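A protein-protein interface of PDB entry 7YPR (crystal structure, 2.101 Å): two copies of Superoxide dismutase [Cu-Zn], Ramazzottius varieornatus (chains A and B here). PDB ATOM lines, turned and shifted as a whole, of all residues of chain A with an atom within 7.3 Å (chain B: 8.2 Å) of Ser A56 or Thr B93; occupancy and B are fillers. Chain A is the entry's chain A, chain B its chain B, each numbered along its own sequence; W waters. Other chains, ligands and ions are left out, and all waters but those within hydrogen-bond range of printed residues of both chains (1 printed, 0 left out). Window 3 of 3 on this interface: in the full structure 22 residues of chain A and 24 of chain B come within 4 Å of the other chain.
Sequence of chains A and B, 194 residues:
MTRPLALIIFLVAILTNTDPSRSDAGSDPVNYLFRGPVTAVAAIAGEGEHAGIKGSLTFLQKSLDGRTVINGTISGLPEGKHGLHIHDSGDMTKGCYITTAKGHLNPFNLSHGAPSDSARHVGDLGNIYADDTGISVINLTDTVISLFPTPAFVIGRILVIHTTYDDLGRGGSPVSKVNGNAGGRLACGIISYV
Water W1 lies within hydrogen-bond range of the backbone NH of Met B92 (2.9 Å), the side-chain hydroxyl of Ser A192 (3.1 Å) and the backbone carbonyl oxygen of Gly B90 (3.1 Å).
O of Gly B90 is in hydrogen-bond range of OG of Ser A192, 2.7 Å away.
OG of Ser B89 is in hydrogen-bond range of OXT of Val A194, 2.6 Å away.
Hydrophobic or aromatic side chains of chain B within 4 Å of the printed part of chain A: Ile B190.
Printed residues of chain A that touch a printed residue of chain B: Val A41, Ala A43, Ser A56, Ser A192 and Val A194.
Along chain A the printed residues that touch a printed residue of chain B span positions 41 to 194.
Among the printed residues, 8 pairs touch across the chains.
Among the printed residues, no Asp or Glu carboxylate lies within 4 Å of a Lys or Arg side-chain nitrogen of the other chain.
No position is printed for both chains.
Of the 8 pairs that touch across the chains among the printed residues, none has its exchanged pair printed and touching as well.
Of the printed residues of chain B, Val A41 touches Asp B91 (3.6 Å).
No residue of chain B comes within 4 Å of Gly A55.
Of the printed residues of chain A, Gly B90 touches Ser A192.
Of the printed residues of chain A, Asp B91 touches Val A41 and Val A194.
Printed residues of chain A within 4 Å of Met B92: Ala A43 (3.7 Å).
Of chain A, only Ala A43 (3.9 Å) and Ser A56 (3.7 Å) come within 4 Å of Thr B93.
Of the printed residues of chain A, Ile B190 touches Ser A192 (3.8 Å).
The nearest printed residue of chain B that does not touch Ser A192 is Asp B91 (4.5 Å).
N of Val A41 is in hydrogen-bond range of O of Ser A192 (2.8 Å).
The backbone NH (N) of Ser A56 is in hydrogen-bond range of the backbone carbonyl oxygen (O) of Thr A73 (3.1 Å).
OG of Ser B89 is in hydrogen-bond range of N of Asp B91 (3.1 Å).
The backbone carbonyl oxygen (O) of Ser B89 is in hydrogen-bond range of the backbone NH (N) of Ile B158.
OD1 of Asp B91 sits at hydrogen-bond distance from OG1 of Thr B93 (2.5 Å).
OG1 of Thr B93 lies within hydrogen-bond range of NZ of Lys B94 (2.9 Å).
Among the printed residues, pairs that only touch across the chains: Val A41 with Asp B91, Ala A43 with Met B92, Ala A43 with Thr B93, Ser A56 with Thr B93, Ser A192 with Ile B190 and Val A194 with Asp B91.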
ATOM      1  N   VAL A  41      -3.090   3.752  26.315  1.00  0.00           N
ATOM      2  CA  VAL A  41      -3.179   2.320  26.056  1.00  0.00           C
ATOM      3  C   VAL A  41      -2.609   2.012  24.680  1.00  0.00           C
ATOM      4  O   VAL A  41      -2.491   2.883  23.818  1.00  0.00           O
ATOM      5  CB  VAL A  41      -4.627   1.779  26.132  1.00  0.00           C
ATOM      6  CG1 VAL A  41      -5.155   1.884  27.533  1.00  0.00           C
ATOM      7  CG2 VAL A  41      -5.542   2.530  25.134  1.00  0.00           C
ATOM      8  N   ALA A  42      -2.279   0.734  24.482  1.00  0.00           N
ATOM      9  CA  ALA A  42      -1.955   0.192  23.168  1.00  0.00           C
ATOM     10  C   ALA A  42      -2.663  -1.144  23.016  1.00  0.00           C
ATOM     11  O   ALA A  42      -2.456  -2.050  23.830  1.00  0.00           O
ATOM     12  CB  ALA A  42      -0.441   0.025  22.986  1.00  0.00           C
ATOM     13  N   ALA A  43      -3.511  -1.247  21.995  1.00  0.00           N
ATOM     14  CA  ALA A  43      -4.049  -2.526  21.539  1.00  0.00           C
ATOM     15  C   ALA A  43      -2.986  -3.230  20.712  1.00  0.00           C
ATOM     16  O   ALA A  43      -2.585  -2.727  19.661  1.00  0.00           O
ATOM     17  CB  ALA A  43      -5.316  -2.314  20.703  1.00  0.00           C
ATOM     18  N   ILE A  44      -2.514  -4.378  21.184  1.00  0.00           N
ATOM     19  CA  ILE A  44      -1.463  -5.129  20.501  1.00  0.00           C
ATOM     20  C   ILE A  44      -2.108  -6.246  19.694  1.00  0.00           C
ATOM     21  O   ILE A  44      -2.957  -6.982  20.212  1.00  0.00           O
ATOM     22  CB  ILE A  44      -0.446  -5.698  21.501  1.00  0.00           C
ATOM     23  CG1 ILE A  44       0.194  -4.567  22.296  1.00  0.00           C
ATOM     24  CG2 ILE A  44       0.593  -6.544  20.776  1.00  0.00           C
ATOM     25  CD1 ILE A  44       0.835  -3.513  21.419  1.00  0.00           C
ATOM     26  N   ALA A  45      -1.710  -6.373  18.429  1.00  0.00           N
ATOM     27  CA  ALA A  45      -2.193  -7.450  17.573  1.00  0.00           C
ATOM     28  C   ALA A  45      -1.135  -7.793  16.528  1.00  0.00           C
ATOM     29  O   ALA A  45      -0.438  -6.901  16.031  1.00  0.00           O
ATOM     30  CB  ALA A  45      -3.501  -7.061  16.874  1.00  0.00           C
ATOM     31  N   LYS A  54      -2.439 -11.345  20.525  1.00  0.00           N
ATOM     32  CA  LYS A  54      -3.396 -10.309  20.892  1.00  0.00           C
ATOM     33  C   LYS A  54      -3.169  -9.902  22.340  1.00  0.00           C
ATOM     34  O   LYS A  54      -2.931 -10.758  23.193  1.00  0.00           O
ATOM     35  CB  LYS A  54      -4.838 -10.808  20.750  1.00  0.00           C
ATOM     36  CG  LYS A  54      -5.216 -11.319  19.359  1.00  0.00           C
ATOM     37  CD  LYS A  54      -5.643 -10.175  18.431  1.00  0.00           C
ATOM     38  CE  LYS A  54      -6.566  -9.181  19.130  1.00  0.00           C
ATOM     39  NZ  LYS A  54      -8.014  -9.558  19.032  1.00  0.00           N
ATOM     40  N   GLY A  55      -3.276  -8.611  22.627  1.00  0.00           N
ATOM     41  CA  GLY A  55      -3.142  -8.171  24.000  1.00  0.00           C
ATOM     42  C   GLY A  55      -3.318  -6.675  24.106  1.00  0.00           C
ATOM     43  O   GLY A  55      -3.705  -5.997  23.150  1.00  0.00           O
ATOM     44  N   SER A  56      -3.010  -6.158  25.286  1.00  0.00           N
ATOM     45  CA  SER A  56      -3.058  -4.718  25.476  1.00  0.00           C
ATOM     46  C   SER A  56      -2.113  -4.329  26.596  1.00  0.00           C
ATOM     47  O   SER A  56      -1.742  -5.147  27.443  1.00  0.00           O
ATOM     48  CB  SER A  56      -4.474  -4.237  25.800  1.00  0.00           C
ATOM     49  OG  SER A  56      -4.958  -4.919  26.945  1.00  0.00           O
ATOM     50  N   LEU A  57      -1.730  -3.059  26.579  1.00  0.00           N
ATOM     51  CA  LEU A  57      -0.898  -2.446  27.594  1.00  0.00           C
ATOM     52  C   LEU A  57      -1.568  -1.155  28.021  1.00  0.00           C
ATOM     53  O   LEU A  57      -2.184  -0.468  27.196  1.00  0.00           O
ATOM     54  CB  LEU A  57       0.510  -2.160  27.053  1.00  0.00           C
ATOM     55  CG  LEU A  57       1.455  -3.360  26.954  1.00  0.00           C
ATOM     56  CD1 LEU A  57       1.099  -4.223  25.757  1.00  0.00           C
ATOM     57  CD2 LEU A  57       2.866  -2.874  26.809  1.00  0.00           C
ATOM     58  N   THR A  58      -1.466  -0.838  29.307  1.00  0.00           N
ATOM     59  CA  THR A  58      -1.895   0.446  29.837  1.00  0.00           C
ATOM     60  C   THR A  58      -0.674   1.174  30.379  1.00  0.00           C
ATOM     61  O   THR A  58       0.145   0.577  31.086  1.00  0.00           O
ATOM     62  CB  THR A  58      -2.939   0.281  30.948  1.00  0.00           C
ATOM     63  OG1 THR A  58      -4.033  -0.497  30.460  1.00  0.00           O
ATOM     64  CG2 THR A  58      -3.479   1.659  31.374  1.00  0.00           C
ATOM     65  N   PHE A  59      -0.563   2.456  30.043  1.00  0.00           N
ATOM     66  CA  PHE A  59       0.508   3.335  30.476  1.00  0.00           C
ATOM     67  C   PHE A  59      -0.093   4.351  31.432  1.00  0.00           C
ATOM     68  O   PHE A  59      -1.103   4.987  31.105  1.00  0.00           O
ATOM     69  CB  PHE A  59       1.138   4.077  29.289  1.00  0.00           C
ATOM     70  CG  PHE A  59       1.824   3.198  28.278  1.00  0.00           C
ATOM     71  CD1 PHE A  59       1.091   2.442  27.367  1.00  0.00           C
ATOM     72  CD2 PHE A  59       3.204   3.173  28.202  1.00  0.00           C
ATOM     73  CE1 PHE A  59       1.736   1.654  26.417  1.00  0.00           C
ATOM     74  CE2 PHE A  59       3.858   2.401  27.245  1.00  0.00           C
ATOM     75  CZ  PHE A  59       3.117   1.618  26.362  1.00  0.00           C
ATOM     76  N   ASN A  71       1.519  -1.801  32.382  1.00  0.00           N
ATOM     77  CA  ASN A  71       0.908  -3.050  32.795  1.00  0.00           C
ATOM     78  C   ASN A  71       0.125  -3.592  31.617  1.00  0.00           C
ATOM     79  O   ASN A  71      -0.476  -2.823  30.869  1.00  0.00           O
ATOM     80  CB  ASN A  71      -0.031  -2.839  33.997  1.00  0.00           C
ATOM     81  CG  ASN A  71       0.719  -2.446  35.270  1.00  0.00           C
ATOM     82  OD1 ASN A  71       0.452  -1.401  35.864  1.00  0.00           O
ATOM     83  ND2 ASN A  71       1.633  -3.284  35.699  1.00  0.00           N
ATOM     84  N   GLY A  72       0.130  -4.904  31.455  1.00  0.00           N
ATOM     85  CA  GLY A  72      -0.710  -5.508  30.441  1.00  0.00           C
ATOM     86  C   GLY A  72      -0.501  -6.999  30.378  1.00  0.00           C
ATOM     87  O   GLY A  72       0.255  -7.589  31.164  1.00  0.00           O
ATOM     88  N   THR A  73      -1.218  -7.608  29.443  1.00  0.00           N
ATOM     89  CA  THR A  73      -1.032  -9.017  29.119  1.00  0.00           C
ATOM     90  C   THR A  73      -1.070  -9.170  27.609  1.00  0.00           C
ATOM     91  O   THR A  73      -1.780  -8.441  26.914  1.00  0.00           O
ATOM     92  CB  THR A  73      -2.106  -9.936  29.734  1.00  0.00           C
ATOM     93  OG1 THR A  73      -3.402  -9.422  29.415  1.00  0.00           O
ATOM     94  CG2 THR A  73      -1.958 -10.036  31.249  1.00  0.00           C
ATOM     95  N   ILE A  74      -0.279 -10.104  27.106  1.00  0.00           N
ATOM     96  CA  ILE A  74      -0.380 -10.535  25.725  1.00  0.00           C
ATOM     97  C   ILE A  74      -0.485 -12.051  25.720  1.00  0.00           C
ATOM     98  O   ILE A  74       0.171 -12.734  26.511  1.00  0.00           O
ATOM     99  CB  ILE A  74       0.812 -10.060  24.873  1.00  0.00           C
ATOM    100  CG1 ILE A  74       1.061  -8.561  25.080  1.00  0.00           C
ATOM    101  CG2 ILE A  74       0.560 -10.389  23.390  1.00  0.00           C
ATOM    102  CD1 ILE A  74       2.272  -8.072  24.350  1.00  0.00           C
ATOM    103  N   SER A  75      -1.344 -12.576  24.866  1.00  0.00           N
ATOM    104  CA  SER A  75      -1.466 -14.011  24.703  1.00  0.00           C
ATOM    105  C   SER A  75      -1.061 -14.387  23.280  1.00  0.00           C
ATOM    106  O   SER A  75      -0.976 -13.532  22.396  1.00  0.00           O
ATOM    107  CB  SER A  75      -2.895 -14.466  25.032  1.00  0.00           C
ATOM    108  OG  SER A  75      -3.808 -13.971  24.079  1.00  0.00           O
ATOM    109  N   SER A 136       2.120 -13.497  28.229  1.00  0.00           N
ATOM    110  CA  SER A 136       3.111 -12.593  28.793  1.00  0.00           C
ATOM    111  C   SER A 136       2.420 -11.607  29.716  1.00  0.00           C
ATOM    112  O   SER A 136       1.448 -10.950  29.322  1.00  0.00           O
ATOM    113  CB  SER A 136       3.881 -11.842  27.702  1.00  0.00           C
ATOM    114  OG  SER A 136       4.810 -10.952  28.297  1.00  0.00           O
ATOM    115  N   ILE A 138       3.003  -8.213  31.412  1.00  0.00           N
ATOM    116  CA  ILE A 138       3.861  -7.043  31.321  1.00  0.00           C
ATOM    117  C   ILE A 138       3.705  -6.245  32.600  1.00  0.00           C
ATOM    118  O   ILE A 138       2.590  -5.905  33.016  1.00  0.00           O
ATOM    119  CB  ILE A 138       3.511  -6.189  30.099  1.00  0.00           C
ATOM    120  CG1 ILE A 138       4.015  -6.877  28.834  1.00  0.00           C
ATOM    121  CG2 ILE A 138       4.119  -4.785  30.250  1.00  0.00           C
ATOM    122  CD1 ILE A 138       2.965  -7.655  28.144  1.00  0.00           C
ATOM    123  N   LEU A 159       4.080   0.881  19.383  1.00  0.00           N
ATOM    124  CA  LEU A 159       4.789  -0.021  20.282  1.00  0.00           C
ATOM    125  C   LEU A 159       4.960  -1.369  19.586  1.00  0.00           C
ATOM    126  O   LEU A 159       4.001  -1.906  19.039  1.00  0.00           O
ATOM    127  CB  LEU A 159       4.022  -0.171  21.595  1.00  0.00           C
ATOM    128  CG  LEU A 159       4.576  -1.157  22.611  1.00  0.00           C
ATOM    129  CD1 LEU A 159       5.479  -0.435  23.589  1.00  0.00           C
ATOM    130  CD2 LEU A 159       3.451  -1.734  23.394  1.00  0.00           C
ATOM    131  N   SER A 192      -2.045   5.378  22.540  1.00  0.00           N
ATOM    132  CA  SER A 192      -2.980   6.484  22.376  1.00  0.00           C
ATOM    133  C   SER A 192      -3.701   6.737  23.679  1.00  0.00           C
ATOM    134  O   SER A 192      -3.528   6.015  24.660  1.00  0.00           O
ATOM    135  CB  SER A 192      -3.978   6.191  21.252  1.00  0.00           C
ATOM    136  OG  SER A 192      -4.536   4.927  21.474  1.00  0.00           O
ATOM    137  N   VAL A 194      -6.506   7.083  26.518  1.00  0.00           N
ATOM    138  CA  VAL A 194      -7.645   6.304  26.967  1.00  0.00           C
ATOM    139  C   VAL A 194      -8.916   7.137  26.799  1.00  0.00           C
ATOM    140  O   VAL A 194      -8.881   8.365  26.937  1.00  0.00           O
ATOM    141  CB  VAL A 194      -7.454   5.852  28.403  1.00  0.00           C
ATOM    142  CG1 VAL A 194      -8.649   5.078  28.876  1.00  0.00           C
ATOM    143  CG2 VAL A 194      -6.264   4.981  28.446  1.00  0.00           C
ATOM    144  OXT VAL A 194      -9.996   6.606  26.503  1.00  0.00           O
ATOM    145  N   SER B  89     -11.931   9.550  22.947  1.00  0.00           N
ATOM    146  CA  SER B  89     -11.076   8.445  23.355  1.00  0.00           C
ATOM    147  C   SER B  89     -10.219   7.974  22.184  1.00  0.00           C
ATOM    148  O   SER B  89     -10.650   7.991  21.029  1.00  0.00           O
ATOM    149  CB  SER B  89     -11.924   7.280  23.889  1.00  0.00           C
ATOM    150  OG  SER B  89     -11.127   6.157  24.251  1.00  0.00           O
ATOM    151  N   GLY B  90      -8.998   7.541  22.486  1.00  0.00           N
ATOM    152  CA  GLY B  90      -8.179   6.834  21.514  1.00  0.00           C
ATOM    153  C   GLY B  90      -8.049   5.354  21.795  1.00  0.00           C
ATOM    154  O   GLY B  90      -7.214   4.686  21.171  1.00  0.00           O
ATOM    155  N   ASP B  91      -8.876   4.802  22.669  1.00  0.00           N
ATOM    156  CA  ASP B  91      -8.703   3.441  23.166  1.00  0.00           C
ATOM    157  C   ASP B  91      -9.320   2.451  22.183  1.00  0.00           C
ATOM    158  O   ASP B  91     -10.547   2.370  22.054  1.00  0.00           O
ATOM    159  CB  ASP B  91      -9.342   3.326  24.547  1.00  0.00           C
ATOM    160  CG  ASP B  91      -9.199   1.936  25.155  1.00  0.00           C
ATOM    161  OD1 ASP B  91      -8.757   0.995  24.453  1.00  0.00           O
ATOM    162  OD2 ASP B  91      -9.504   1.797  26.360  1.00  0.00           O
ATOM    163  N   MET B  92      -8.474   1.673  21.513  1.00  0.00           N
ATOM    164  CA  MET B  92      -8.923   0.635  20.601  1.00  0.00           C
ATOM    165  C   MET B  92      -8.894  -0.747  21.220  1.00  0.00           C
ATOM    166  O   MET B  92      -9.010  -1.732  20.487  1.00  0.00           O
ATOM    167  CB  MET B  92      -8.065   0.631  19.332  1.00  0.00           C
ATOM    168  CG  MET B  92      -8.371   1.806  18.411  1.00  0.00           C
ATOM    169  SD  MET B  92     -10.000   1.584  17.696  1.00  0.00           S
ATOM    170  CE  MET B  92      -9.696   0.120  16.700  1.00  0.00           C
ATOM    171  N   THR B  93      -8.720  -0.852  22.541  1.00  0.00           N
ATOM    172  CA  THR B  93      -8.491  -2.167  23.133  1.00  0.00           C
ATOM    173  C   THR B  93      -9.758  -2.997  23.227  1.00  0.00           C
ATOM    174  O   THR B  93      -9.661  -4.192  23.517  1.00  0.00           O
ATOM    175  CB  THR B  93      -7.871  -2.069  24.544  1.00  0.00           C
ATOM    176  OG1 THR B  93      -8.720  -1.309  25.406  1.00  0.00           O
ATOM    177  CG2 THR B  93      -6.471  -1.424  24.526  1.00  0.00           C
ATOM    178  N   LYS B  94     -10.942  -2.400  23.033  1.00  0.00           N
ATOM    179  CA  LYS B  94     -12.185  -3.167  22.965  1.00  0.00           C
ATOM    180  C   LYS B  94     -12.720  -3.239  21.546  1.00  0.00           C
ATOM    181  O   LYS B  94     -13.906  -3.503  21.349  1.00  0.00           O
ATOM    182  CB  LYS B  94     -13.264  -2.595  23.892  1.00  0.00           C
ATOM    183  CG  LYS B  94     -12.792  -2.199  25.291  1.00  0.00           C
ATOM    184  CD  LYS B  94     -12.503  -0.704  25.388  1.00  0.00           C
ATOM    185  CE  LYS B  94     -12.198  -0.263  26.825  1.00  0.00           C
ATOM    186  NZ  LYS B  94     -10.763  -0.477  27.211  1.00  0.00           N
ATOM    187  N   GLY B  95     -11.870  -3.007  20.552  1.00  0.00           N
ATOM    188  CA  GLY B  95     -12.308  -2.996  19.178  1.00  0.00           C
ATOM    189  C   GLY B  95     -12.977  -1.692  18.788  1.00  0.00           C
ATOM    190  O   GLY B  95     -13.199  -0.783  19.590  1.00  0.00           O
ATOM    191  N   CYS B  96     -13.310  -1.588  17.505  1.00  0.00           N
ATOM    192  CA  CYS B  96     -13.888  -0.338  17.030  1.00  0.00           C
ATOM    193  C   CYS B  96     -15.372  -0.224  17.364  1.00  0.00           C
ATOM    194  O   CYS B  96     -15.863   0.887  17.592  1.00  0.00           O
ATOM    195  CB  CYS B  96     -13.660  -0.198  15.521  1.00  0.00           C
ATOM    196  SG  CYS B  96     -14.649   1.088  14.685  1.00  0.00           S
ATOM    197  N   ILE B  98     -17.477  -0.697  19.794  1.00  0.00           N
ATOM    198  CA  ILE B  98     -18.085  -0.442  21.085  1.00  0.00           C
ATOM    199  C   ILE B  98     -19.173   0.633  20.968  1.00  0.00           C
ATOM    200  O   ILE B  98     -19.179   1.462  20.049  1.00  0.00           O
ATOM    201  CB  ILE B  98     -16.982  -0.021  22.064  1.00  0.00           C
ATOM    202  CG1 ILE B  98     -16.268   1.225  21.539  1.00  0.00           C
ATOM    203  CG2 ILE B  98     -15.974  -1.131  22.172  1.00  0.00           C
ATOM    204  CD1 ILE B  98     -15.183   1.732  22.454  1.00  0.00           C
ATOM    205  N   ILE B 158      -9.356   8.523  18.332  1.00  0.00           N
ATOM    206  CA  ILE B 158      -9.916   7.676  17.284  1.00  0.00           C
ATOM    207  C   ILE B 158     -10.735   8.539  16.340  1.00  0.00           C
ATOM    208  O   ILE B 158     -11.575   9.330  16.784  1.00  0.00           O
ATOM    209  CB  ILE B 158     -10.767   6.544  17.878  1.00  0.00           C
ATOM    210  CG1 ILE B 158      -9.868   5.422  18.416  1.00  0.00           C
ATOM    211  CG2 ILE B 158     -11.713   5.957  16.829  1.00  0.00           C
ATOM    212  CD1 ILE B 158     -10.516   4.694  19.570  1.00  0.00           C
ATOM    213  N   ILE B 190      -6.862   5.229  14.634  1.00  0.00           N
ATOM    214  CA  ILE B 190      -6.202   6.148  15.559  1.00  0.00           C
ATOM    215  C   ILE B 190      -5.386   7.154  14.763  1.00  0.00           C
ATOM    216  O   ILE B 190      -4.623   6.791  13.862  1.00  0.00           O
ATOM    217  CB  ILE B 190      -5.299   5.381  16.543  1.00  0.00           C
ATOM    218  CG1 ILE B 190      -6.105   4.404  17.383  1.00  0.00           C
ATOM    219  CG2 ILE B 190      -4.583   6.337  17.498  1.00  0.00           C
ATOM    220  CD1 ILE B 190      -5.219   3.315  18.018  1.00  0.00           C
HETATM  221  O   HOH W   1      -5.638   2.052  21.429  1.00  0.00           O
